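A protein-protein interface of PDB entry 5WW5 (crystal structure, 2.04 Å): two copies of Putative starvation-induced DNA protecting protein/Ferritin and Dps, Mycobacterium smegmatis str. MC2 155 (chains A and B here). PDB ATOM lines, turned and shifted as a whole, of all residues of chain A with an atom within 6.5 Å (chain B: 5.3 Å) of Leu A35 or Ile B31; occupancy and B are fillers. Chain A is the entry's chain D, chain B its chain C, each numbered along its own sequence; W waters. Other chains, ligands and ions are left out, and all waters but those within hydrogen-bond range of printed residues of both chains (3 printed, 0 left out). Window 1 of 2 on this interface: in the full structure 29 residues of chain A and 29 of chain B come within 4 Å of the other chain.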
ATOM      1  N   LEU A  30      -0.776  27.231   4.418  1.00  0.00           N
ATOM      2  CA  LEU A  30      -1.612  27.278   5.636  1.00  0.00           C
ATOM      3  C   LEU A  30      -1.705  25.919   6.343  1.00  0.00           C
ATOM      4  O   LEU A  30      -1.618  25.853   7.573  1.00  0.00           O
ATOM      5  CB  LEU A  30      -3.019  27.823   5.334  1.00  0.00           C
ATOM      6  CG  LEU A  30      -3.161  29.341   5.120  1.00  0.00           C
ATOM      7  CD1 LEU A  30      -4.548  29.653   4.567  1.00  0.00           C
ATOM      8  CD2 LEU A  30      -2.885  30.150   6.395  1.00  0.00           C
ATOM      9  N   ILE A  31      -1.886  24.850   5.563  1.00  0.00           N
ATOM     10  CA  ILE A  31      -1.914  23.483   6.109  1.00  0.00           C
ATOM     11  C   ILE A  31      -0.540  23.089   6.664  1.00  0.00           C
ATOM     12  O   ILE A  31      -0.453  22.607   7.790  1.00  0.00           O
ATOM     13  CB  ILE A  31      -2.442  22.440   5.098  1.00  0.00           C
ATOM     14  CG1 ILE A  31      -3.910  22.731   4.744  1.00  0.00           C
ATOM     15  CG2 ILE A  31      -2.336  21.021   5.669  1.00  0.00           C
ATOM     16  CD1 ILE A  31      -4.409  21.971   3.536  1.00  0.00           C
ATOM     17  N   GLU A  32       0.522  23.330   5.891  1.00  0.00           N
ATOM     18  CA  GLU A  32       1.887  23.086   6.370  1.00  0.00           C
ATOM     19  C   GLU A  32       2.186  23.852   7.664  1.00  0.00           C
ATOM     20  O   GLU A  32       2.766  23.289   8.602  1.00  0.00           O
ATOM     21  CB  GLU A  32       2.931  23.397   5.291  1.00  0.00           C
ATOM     22  CG  GLU A  32       4.385  23.134   5.701  1.00  0.00           C
ATOM     23  CD  GLU A  32       4.716  21.661   5.937  1.00  0.00           C
ATOM     24  OE1 GLU A  32       5.844  21.392   6.408  1.00  0.00           O
ATOM     25  OE2 GLU A  32       3.874  20.773   5.657  1.00  0.00           O
ATOM     26  N   LEU A  33       1.768  25.116   7.720  1.00  0.00           N
ATOM     27  CA  LEU A  33       1.938  25.914   8.936  1.00  0.00           C
ATOM     28  C   LEU A  33       1.220  25.315  10.155  1.00  0.00           C
ATOM     29  O   LEU A  33       1.789  25.304  11.262  1.00  0.00           O
ATOM     30  CB  LEU A  33       1.528  27.372   8.707  1.00  0.00           C
ATOM     31  CG  LEU A  33       1.769  28.382   9.835  1.00  0.00           C
ATOM     32  CD1 LEU A  33       3.251  28.529  10.171  1.00  0.00           C
ATOM     33  CD2 LEU A  33       1.184  29.725   9.434  1.00  0.00           C
ATOM     34  N   SER A  34      -0.005  24.817   9.938  1.00  0.00           N
ATOM     35  CA  SER A  34      -0.802  24.166  10.990  1.00  0.00           C
ATOM     36  C   SER A  34      -0.114  22.910  11.522  1.00  0.00           C
ATOM     37  O   SER A  34      -0.097  22.669  12.723  1.00  0.00           O
ATOM     38  CB  SER A  34      -2.201  23.806  10.479  1.00  0.00           C
ATOM     39  OG  SER A  34      -2.915  24.950  10.064  1.00  0.00           O
ATOM     40  N   LEU A  35       0.450  22.110  10.605  1.00  0.00           N
ATOM     41  CA  LEU A  35       1.185  20.874  10.950  1.00  0.00           C
ATOM     42  C   LEU A  35       2.515  21.161  11.675  1.00  0.00           C
ATOM     43  O   LEU A  35       2.860  20.483  12.655  1.00  0.00           O
ATOM     44  CB  LEU A  35       1.422  20.010   9.693  1.00  0.00           C
ATOM     45  CG  LEU A  35       0.206  19.390   8.971  1.00  0.00           C
ATOM     46  CD1 LEU A  35       0.576  18.863   7.587  1.00  0.00           C
ATOM     47  CD2 LEU A  35      -0.460  18.295   9.798  1.00  0.00           C
ATOM     48  N   GLN A  36       3.248  22.168  11.195  1.00  0.00           N
ATOM     49  CA  GLN A  36       4.489  22.602  11.847  1.00  0.00           C
ATOM     50  C   GLN A  36       4.209  23.233  13.221  1.00  0.00           C
ATOM     51  O   GLN A  36       4.940  22.983  14.177  1.00  0.00           O
ATOM     52  CB  GLN A  36       5.289  23.552  10.946  1.00  0.00           C
ATOM     53  CG  GLN A  36       5.821  22.883   9.677  1.00  0.00           C
ATOM     54  CD  GLN A  36       6.996  23.607   9.047  1.00  0.00           C
ATOM     55  OE1 GLN A  36       7.731  24.305   9.728  1.00  0.00           O
ATOM     56  NE2 GLN A  36       7.200  23.415   7.741  1.00  0.00           N
ATOM     57  N   GLY A  37       3.143  24.029  13.305  1.00  0.00           N
ATOM     58  CA  GLY A  37       2.709  24.647  14.563  1.00  0.00           C
ATOM     59  C   GLY A  37       2.451  23.617  15.652  1.00  0.00           C
ATOM     60  O   GLY A  37       2.900  23.793  16.795  1.00  0.00           O
ATOM     61  N   LYS A  38       1.734  22.547  15.296  1.00  0.00           N
ATOM     62  CA  LYS A  38       1.449  21.435  16.224  1.00  0.00           C
ATOM     63  C   LYS A  38       2.710  20.689  16.647  1.00  0.00           C
ATOM     64  O   LYS A  38       2.891  20.400  17.838  1.00  0.00           O
ATOM     65  CB  LYS A  38       0.412  20.459  15.636  1.00  0.00           C
ATOM     66  CG  LYS A  38      -1.048  20.820  15.929  1.00  0.00           C
ATOM     67  CD  LYS A  38      -1.340  20.823  17.434  1.00  0.00           C
ATOM     68  CE  LYS A  38      -2.820  20.972  17.727  1.00  0.00           C
ATOM     69  NZ  LYS A  38      -3.074  21.098  19.192  1.00  0.00           N
ATOM     70  N   GLN A  39       3.572  20.389  15.675  1.00  0.00           N
ATOM     71  CA  GLN A  39       4.894  19.801  15.932  1.00  0.00           C
ATOM     72  C   GLN A  39       5.690  20.621  16.966  1.00  0.00           C
ATOM     73  O   GLN A  39       6.223  20.058  17.937  1.00  0.00           O
ATOM     74  CB  GLN A  39       5.678  19.658  14.614  1.00  0.00           C
ATOM     75  CG  GLN A  39       7.058  19.014  14.743  1.00  0.00           C
ATOM     76  CD  GLN A  39       7.023  17.507  14.897  1.00  0.00           C
ATOM     77  OE1 GLN A  39       5.973  16.874  14.770  1.00  0.00           O
ATOM     78  NE2 GLN A  39       8.187  16.916  15.165  1.00  0.00           N
ATOM     79  N   ALA A  40       5.738  21.939  16.755  1.00  0.00           N
ATOM     80  CA  ALA A  40       6.372  22.894  17.680  1.00  0.00           C
ATOM     81  C   ALA A  40       5.679  22.921  19.050  1.00  0.00           C
ATOM     82  O   ALA A  40       6.342  22.855  20.084  1.00  0.00           O
ATOM     83  CB  ALA A  40       6.404  24.292  17.066  1.00  0.00           C
ATOM     84  N   TRP A  42       3.966  20.541  20.490  1.00  0.00           N
ATOM     85  CA  TRP A  42       4.287  19.305  21.221  1.00  0.00           C
ATOM     86  C   TRP A  42       5.711  19.232  21.754  1.00  0.00           C
ATOM     87  O   TRP A  42       5.928  18.783  22.891  1.00  0.00           O
ATOM     88  CB  TRP A  42       4.002  18.053  20.378  1.00  0.00           C
ATOM     89  CG  TRP A  42       2.567  17.899  19.938  1.00  0.00           C
ATOM     90  CD1 TRP A  42       1.435  18.149  20.680  1.00  0.00           C
ATOM     91  CD2 TRP A  42       2.116  17.431  18.666  1.00  0.00           C
ATOM     92  NE1 TRP A  42       0.308  17.882  19.936  1.00  0.00           N
ATOM     93  CE2 TRP A  42       0.692  17.443  18.694  1.00  0.00           C
ATOM     94  CE3 TRP A  42       2.775  17.021  17.490  1.00  0.00           C
ATOM     95  CZ2 TRP A  42      -0.090  17.046  17.593  1.00  0.00           C
ATOM     96  CZ3 TRP A  42       1.999  16.630  16.389  1.00  0.00           C
ATOM     97  CH2 TRP A  42       0.575  16.646  16.452  1.00  0.00           C
ATOM     98  N   VAL A  60      -2.045  27.615  15.393  1.00  0.00           N
ATOM     99  CA  VAL A  60      -2.672  26.465  14.733  1.00  0.00           C
ATOM    100  C   VAL A  60      -4.185  26.660  14.513  1.00  0.00           C
ATOM    101  O   VAL A  60      -4.677  26.399  13.414  1.00  0.00           O
ATOM    102  CB  VAL A  60      -2.374  25.119  15.458  1.00  0.00           C
ATOM    103  CG1 VAL A  60      -3.115  23.958  14.808  1.00  0.00           C
ATOM    104  CG2 VAL A  60      -0.886  24.814  15.421  1.00  0.00           C
ATOM    105  N   ARG A  64      -5.703  26.784  10.760  1.00  0.00           N
ATOM    106  CA  ARG A  64      -6.751  25.800  10.434  1.00  0.00           C
ATOM    107  C   ARG A  64      -8.045  26.438   9.933  1.00  0.00           C
ATOM    108  O   ARG A  64      -8.599  25.992   8.920  1.00  0.00           O
ATOM    109  CB  ARG A  64      -7.040  24.880  11.624  1.00  0.00           C
ATOM    110  CG  ARG A  64      -6.031  23.753  11.792  1.00  0.00           C
ATOM    111  CD  ARG A  64      -6.262  23.041  13.114  1.00  0.00           C
ATOM    112  NE  ARG A  64      -5.457  21.828  13.267  1.00  0.00           N
ATOM    113  CZ  ARG A  64      -5.381  21.109  14.388  1.00  0.00           C
ATOM    114  NH1 ARG A  64      -6.054  21.479  15.482  1.00  0.00           N
ATOM    115  NH2 ARG A  64      -4.623  20.018  14.424  1.00  0.00           N
ATOM    116  N   SER A  85      -1.776  15.161   2.402  1.00  0.00           N
ATOM    117  CA  SER A  85      -0.415  15.179   2.967  1.00  0.00           C
ATOM    118  C   SER A  85       0.694  15.197   1.900  1.00  0.00           C
ATOM    119  O   SER A  85       1.619  16.001   1.993  1.00  0.00           O
ATOM    120  CB  SER A  85      -0.211  14.006   3.933  1.00  0.00           C
ATOM    121  OG  SER A  85      -0.373  12.762   3.268  1.00  0.00           O
ATOM    122  N   VAL A  88       0.688  18.591   0.126  1.00  0.00           N
ATOM    123  CA  VAL A  88       1.217  19.604   1.047  1.00  0.00           C
ATOM    124  C   VAL A  88       2.754  19.511   1.144  1.00  0.00           C
ATOM    125  O   VAL A  88       3.436  20.517   0.957  1.00  0.00           O
ATOM    126  CB  VAL A  88       0.515  19.575   2.444  1.00  0.00           C
ATOM    127  CG1 VAL A  88       1.201  20.506   3.442  1.00  0.00           C
ATOM    128  CG2 VAL A  88      -0.949  19.961   2.313  1.00  0.00           C
ATOM    129  N   VAL B  26       0.089   5.262  15.594  1.00  0.00           N
ATOM    130  CA  VAL B  26      -1.271   5.779  15.792  1.00  0.00           C
ATOM    131  C   VAL B  26      -1.353   7.250  15.375  1.00  0.00           C
ATOM    132  O   VAL B  26      -2.282   7.645  14.666  1.00  0.00           O
ATOM    133  CB  VAL B  26      -1.768   5.572  17.246  1.00  0.00           C
ATOM    134  CG1 VAL B  26      -3.103   6.275  17.479  1.00  0.00           C
ATOM    135  CG2 VAL B  26      -1.932   4.084  17.537  1.00  0.00           C
ATOM    136  N   LEU B  27      -0.367   8.040  15.806  1.00  0.00           N
ATOM    137  CA  LEU B  27      -0.334   9.472  15.530  1.00  0.00           C
ATOM    138  C   LEU B  27      -0.423   9.812  14.039  1.00  0.00           C
ATOM    139  O   LEU B  27      -1.246  10.641  13.650  1.00  0.00           O
ATOM    140  CB  LEU B  27       0.913  10.120  16.150  1.00  0.00           C
ATOM    141  CG  LEU B  27       1.050  11.636  15.941  1.00  0.00           C
ATOM    142  CD1 LEU B  27      -0.073  12.416  16.614  1.00  0.00           C
ATOM    143  CD2 LEU B  27       2.402  12.120  16.426  1.00  0.00           C
ATOM    144  N   VAL B  28       0.406   9.168  13.211  1.00  0.00           N
ATOM    145  CA  VAL B  28       0.440   9.508  11.776  1.00  0.00           C
ATOM    146  C   VAL B  28      -0.854   9.142  11.075  1.00  0.00           C
ATOM    147  O   VAL B  28      -1.283   9.851  10.165  1.00  0.00           O
ATOM    148  CB  VAL B  28       1.678   8.965  10.999  1.00  0.00           C
ATOM    149  CG1 VAL B  28       2.959   9.610  11.517  1.00  0.00           C
ATOM    150  CG2 VAL B  28       1.765   7.439  11.040  1.00  0.00           C
ATOM    151  N   ASP B  29      -1.476   8.049  11.516  1.00  0.00           N
ATOM    152  CA  ASP B  29      -2.744   7.629  10.938  1.00  0.00           C
ATOM    153  C   ASP B  29      -3.913   8.527  11.346  1.00  0.00           C
ATOM    154  O   ASP B  29      -4.822   8.744  10.544  1.00  0.00           O
ATOM    155  CB  ASP B  29      -3.006   6.147  11.201  1.00  0.00           C
ATOM    156  CG  ASP B  29      -2.194   5.235  10.270  1.00  0.00           C
ATOM    157  OD1 ASP B  29      -1.507   5.719   9.346  1.00  0.00           O
ATOM    158  OD2 ASP B  29      -2.257   4.016  10.450  1.00  0.00           O
ATOM    159  N   LEU B  30      -3.861   9.082  12.564  1.00  0.00           N
ATOM    160  CA  LEU B  30      -4.858  10.074  13.002  1.00  0.00           C
ATOM    161  C   LEU B  30      -4.724  11.415  12.247  1.00  0.00           C
ATOM    162  O   LEU B  30      -5.732  12.038  11.866  1.00  0.00           O
ATOM    163  CB  LEU B  30      -4.777  10.303  14.516  1.00  0.00           C
ATOM    164  CG  LEU B  30      -5.327   9.228  15.464  1.00  0.00           C
ATOM    165  CD1 LEU B  30      -4.921   9.570  16.887  1.00  0.00           C
ATOM    166  CD2 LEU B  30      -6.846   9.102  15.357  1.00  0.00           C
ATOM    167  N   ILE B  31      -3.483  11.848  12.037  1.00  0.00           N
ATOM    168  CA  ILE B  31      -3.208  13.088  11.302  1.00  0.00           C
ATOM    169  C   ILE B  31      -3.623  12.922   9.837  1.00  0.00           C
ATOM    170  O   ILE B  31      -4.314  13.786   9.292  1.00  0.00           O
ATOM    171  CB  ILE B  31      -1.731  13.547  11.415  1.00  0.00           C
ATOM    172  CG1 ILE B  31      -1.405  13.961  12.851  1.00  0.00           C
ATOM    173  CG2 ILE B  31      -1.459  14.724  10.474  1.00  0.00           C
ATOM    174  CD1 ILE B  31       0.079  14.003  13.157  1.00  0.00           C
ATOM    175  N   GLU B  32      -3.217  11.805   9.226  1.00  0.00           N
ATOM    176  CA  GLU B  32      -3.622  11.490   7.852  1.00  0.00           C
ATOM    177  C   GLU B  32      -5.141  11.471   7.699  1.00  0.00           C
ATOM    178  O   GLU B  32      -5.676  12.070   6.762  1.00  0.00           O
ATOM    179  CB  GLU B  32      -3.003  10.172   7.360  1.00  0.00           C
ATOM    180  CG  GLU B  32      -3.388   9.773   5.929  1.00  0.00           C
ATOM    181  CD  GLU B  32      -2.903  10.738   4.841  1.00  0.00           C
ATOM    182  OE1 GLU B  32      -2.091  11.646   5.109  1.00  0.00           O
ATOM    183  OE2 GLU B  32      -3.336  10.577   3.682  1.00  0.00           O
ATOM    184  N   LEU B  33      -5.824  10.796   8.621  1.00  0.00           N
ATOM    185  CA  LEU B  33      -7.296  10.759   8.633  1.00  0.00           C
ATOM    186  C   LEU B  33      -7.928  12.156   8.707  1.00  0.00           C
ATOM    187  O   LEU B  33      -8.904  12.428   7.991  1.00  0.00           O
ATOM    188  CB  LEU B  33      -7.823   9.847   9.753  1.00  0.00           C
ATOM    189  CG  LEU B  33      -9.338   9.600   9.838  1.00  0.00           C
ATOM    190  CD1 LEU B  33      -9.909   8.971   8.566  1.00  0.00           C
ATOM    191  CD2 LEU B  33      -9.643   8.744  11.060  1.00  0.00           C
ATOM    192  N   SER B  34      -7.363  13.021   9.553  1.00  0.00           N
ATOM    193  CA  SER B  34      -7.850  14.393   9.681  1.00  0.00           C
ATOM    194  C   SER B  34      -7.680  15.183   8.376  1.00  0.00           C
ATOM    195  O   SER B  34      -8.562  15.941   8.005  1.00  0.00           O
ATOM    196  CB  SER B  34      -7.188  15.113  10.861  1.00  0.00           C
ATOM    197  OG  SER B  34      -5.812  15.333  10.630  1.00  0.00           O
ATOM    198  N   LEU B  35      -6.556  14.980   7.685  1.00  0.00           N
ATOM    199  CA  LEU B  35      -6.275  15.657   6.413  1.00  0.00           C
ATOM    200  C   LEU B  35      -7.177  15.138   5.297  1.00  0.00           C
ATOM    201  O   LEU B  35      -7.696  15.928   4.503  1.00  0.00           O
ATOM    202  CB  LEU B  35      -4.790  15.532   6.027  1.00  0.00           C
ATOM    203  CG  LEU B  35      -3.748  16.255   6.905  1.00  0.00           C
ATOM    204  CD1 LEU B  35      -2.347  15.796   6.530  1.00  0.00           C
ATOM    205  CD2 LEU B  35      -3.844  17.778   6.795  1.00  0.00           C
ATOM    206  N   GLN B  36      -7.376  13.819   5.258  1.00  0.00           N
ATOM    207  CA  GLN B  36      -8.302  13.208   4.297  1.00  0.00           C
ATOM    208  C   GLN B  36      -9.758  13.587   4.581  1.00  0.00           C
ATOM    209  O   GLN B  36     -10.541  13.801   3.659  1.00  0.00           O
ATOM    210  CB  GLN B  36      -8.157  11.692   4.297  1.00  0.00           C
ATOM    211  CG  GLN B  36      -6.836  11.183   3.741  1.00  0.00           C
ATOM    212  CD  GLN B  36      -6.797   9.668   3.681  1.00  0.00           C
ATOM    213  OE1 GLN B  36      -5.851   9.072   3.166  1.00  0.00           O
ATOM    214  NE2 GLN B  36      -7.810   9.037   4.247  1.00  0.00           N
ATOM    215  N   SER B  67      -5.194  13.077  17.806  1.00  0.00           N
ATOM    216  CA  SER B  67      -3.770  13.227  17.506  1.00  0.00           C
ATOM    217  C   SER B  67      -3.060  13.996  18.622  1.00  0.00           C
ATOM    218  O   SER B  67      -1.959  13.611  19.025  1.00  0.00           O
ATOM    219  CB  SER B  67      -3.548  13.887  16.139  1.00  0.00           C
ATOM    220  OG  SER B  67      -4.141  15.166  16.078  1.00  0.00           O
ATOM    221  N   ASP B  82       6.331  12.766  15.856  1.00  0.00           N
ATOM    222  CA  ASP B  82       6.637  13.405  14.593  1.00  0.00           C
ATOM    223  C   ASP B  82       5.375  13.460  13.746  1.00  0.00           C
ATOM    224  O   ASP B  82       4.969  12.460  13.141  1.00  0.00           O
ATOM    225  CB  ASP B  82       7.781  12.687  13.862  1.00  0.00           C
ATOM    226  CG  ASP B  82       8.200  13.398  12.577  1.00  0.00           C
ATOM    227  OD1 ASP B  82       7.629  14.460  12.221  1.00  0.00           O
ATOM    228  OD2 ASP B  82       9.117  12.887  11.907  1.00  0.00           O
ATOM    229  N   GLY B  83       4.772  14.645  13.714  1.00  0.00           N
ATOM    230  CA  GLY B  83       3.551  14.891  12.933  1.00  0.00           C
ATOM    231  C   GLY B  83       3.743  15.738  11.685  1.00  0.00           C
ATOM    232  O   GLY B  83       2.778  16.283  11.153  1.00  0.00           O
ATOM    233  N   ARG B  84       4.987  15.839  11.210  1.00  0.00           N
ATOM    234  CA  ARG B  84       5.299  16.662  10.035  1.00  0.00           C
ATOM    235  C   ARG B  84       4.761  16.003   8.763  1.00  0.00           C
ATOM    236  O   ARG B  84       4.668  14.772   8.692  1.00  0.00           O
ATOM    237  CB  ARG B  84       6.803  16.909   9.933  1.00  0.00           C
ATOM    238  CG  ARG B  84       7.382  17.635  11.140  1.00  0.00           C
ATOM    239  CD  ARG B  84       8.901  17.614  11.130  1.00  0.00           C
ATOM    240  NE  ARG B  84       9.458  16.254  11.109  1.00  0.00           N
ATOM    241  CZ  ARG B  84      10.710  15.954  10.742  1.00  0.00           C
ATOM    242  NH1 ARG B  84      11.545  16.916  10.365  1.00  0.00           N
ATOM    243  NH2 ARG B  84      11.125  14.684  10.743  1.00  0.00           N
ATOM    244  N   SER B  85       4.408  16.830   7.779  1.00  0.00           N
ATOM    245  CA  SER B  85       3.771  16.378   6.543  1.00  0.00           C
ATOM    246  C   SER B  85       4.539  15.279   5.799  1.00  0.00           C
ATOM    247  O   SER B  85       3.929  14.303   5.375  1.00  0.00           O
ATOM    248  CB  SER B  85       3.489  17.560   5.615  1.00  0.00           C
ATOM    249  OG  SER B  85       4.693  18.258   5.320  1.00  0.00           O
ATOM    250  N   VAL B  88       4.177  12.011   7.828  1.00  0.00           N
ATOM    251  CA  VAL B  88       2.805  11.506   7.704  1.00  0.00           C
ATOM    252  C   VAL B  88       2.635  10.830   6.337  1.00  0.00           C
ATOM    253  O   VAL B  88       2.252   9.661   6.283  1.00  0.00           O
ATOM    254  CB  VAL B  88       1.753  12.608   7.993  1.00  0.00           C
ATOM    255  CG1 VAL B  88       0.339  12.148   7.647  1.00  0.00           C
ATOM    256  CG2 VAL B  88       1.819  13.013   9.463  1.00  0.00           C
HETATM  257  O   HOH W   1       4.970  19.622   8.513  1.00  0.00           O
HETATM  258  O   HOH W   2       1.473  17.846  12.953  1.00  0.00           O
HETATM  259  O   HOH W   3      -4.069  13.359   3.169  1.00  0.00           O
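Among the printed residues, pairs that only touch across the chains: Gln A39 with Asp B82, Ile A31 with Leu B35, Leu A35 with Ser B85, Leu A35 with Ile B31, Gln A39 with Arg B84 and Ser A85 with Leu B35.
The side-chain carboxylate (OE2) of Glu B32 lies close to the side-chain amide oxygen (OE1) of Gln B36 (3.0 Å).
The side-chain amide nitrogen of Gln A36 lies within hydrogen-bond range of the side-chain carboxylate of Glu A32.
The guanidinium group (NE) of Arg B84 is in salt-bridge range of the side-chain carboxylate (OD1) of Asp B82.
The side-chain hydroxyl (OG) of Ser B34 lies within hydrogen-bond range of the backbone carbonyl oxygen (O) of Ile B31, at 2.5 Å.
Of the 17 printed residues of chain B, 7 touch a printed residue of chain A.
Of the 16 printed residues of chain A, 5 touch a printed residue of chain B.
Hydrophobic or aromatic side chains of chain A that line the printed part of chain B: Ile A31 and Leu A35.
Among the printed residues, 9 pairs touch across the chains.
Of chain B, only Ile B31 and Ser B85 come within 4 Å of Leu A35.
Of the printed residues of chain B, Ile A31 touches Leu B35.
Of the printed residues of chain A, Glu B32 touches Ser A85.
Of the printed residues of chain B, Gln A39 touches Asp B82 (3.5 Å), Gly B83 (2.7 Å) and Arg B84 (3.8 Å).
Lys A38 touches none of the printed residues of chain B.
Trp A42 touches none of the printed residues of chain B.
The nearest residue of chain B that does not touch Leu A35 is Gly B83 (4.05 Å).
The nearest residue of chain A that does not touch Ile B31 is Trp A42 (4.3 Å).
Ile A31 touches Leu B35, and with the chains exchanged Leu A35 touches Ile B31.
Glu A32 touches Ser B85, and with the chains exchanged Ser A85 touches Glu B32.
Leu A35 touches Ser B85, and with the chains exchanged Ser A85 touches Leu B35.
9 positions are printed for both chains.
Water W2 lies within hydrogen-bond range of O of Gly B83 and O of Leu A35.
Water W1 lies within hydrogen-bond range of the side-chain carboxylate (OE1) of Glu A32 (2.9 Å) and the backbone NH (N) of Ser B85 (2.9 Å).
Water W3 bridges the side-chain carboxylate of Glu B32 and the backbone NH of Ser A85.
OE2 of Glu A32 is in hydrogen-bond range of OG of Ser B85.
The backbone NH of Gly B83 sits at hydrogen-bond distance from the side-chain amide oxygen of Gln A39 (2.7 Å).
The side-chain carboxylate of Glu B32 sits at hydrogen-bond distance from the side-chain hydroxyl of Ser A85.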
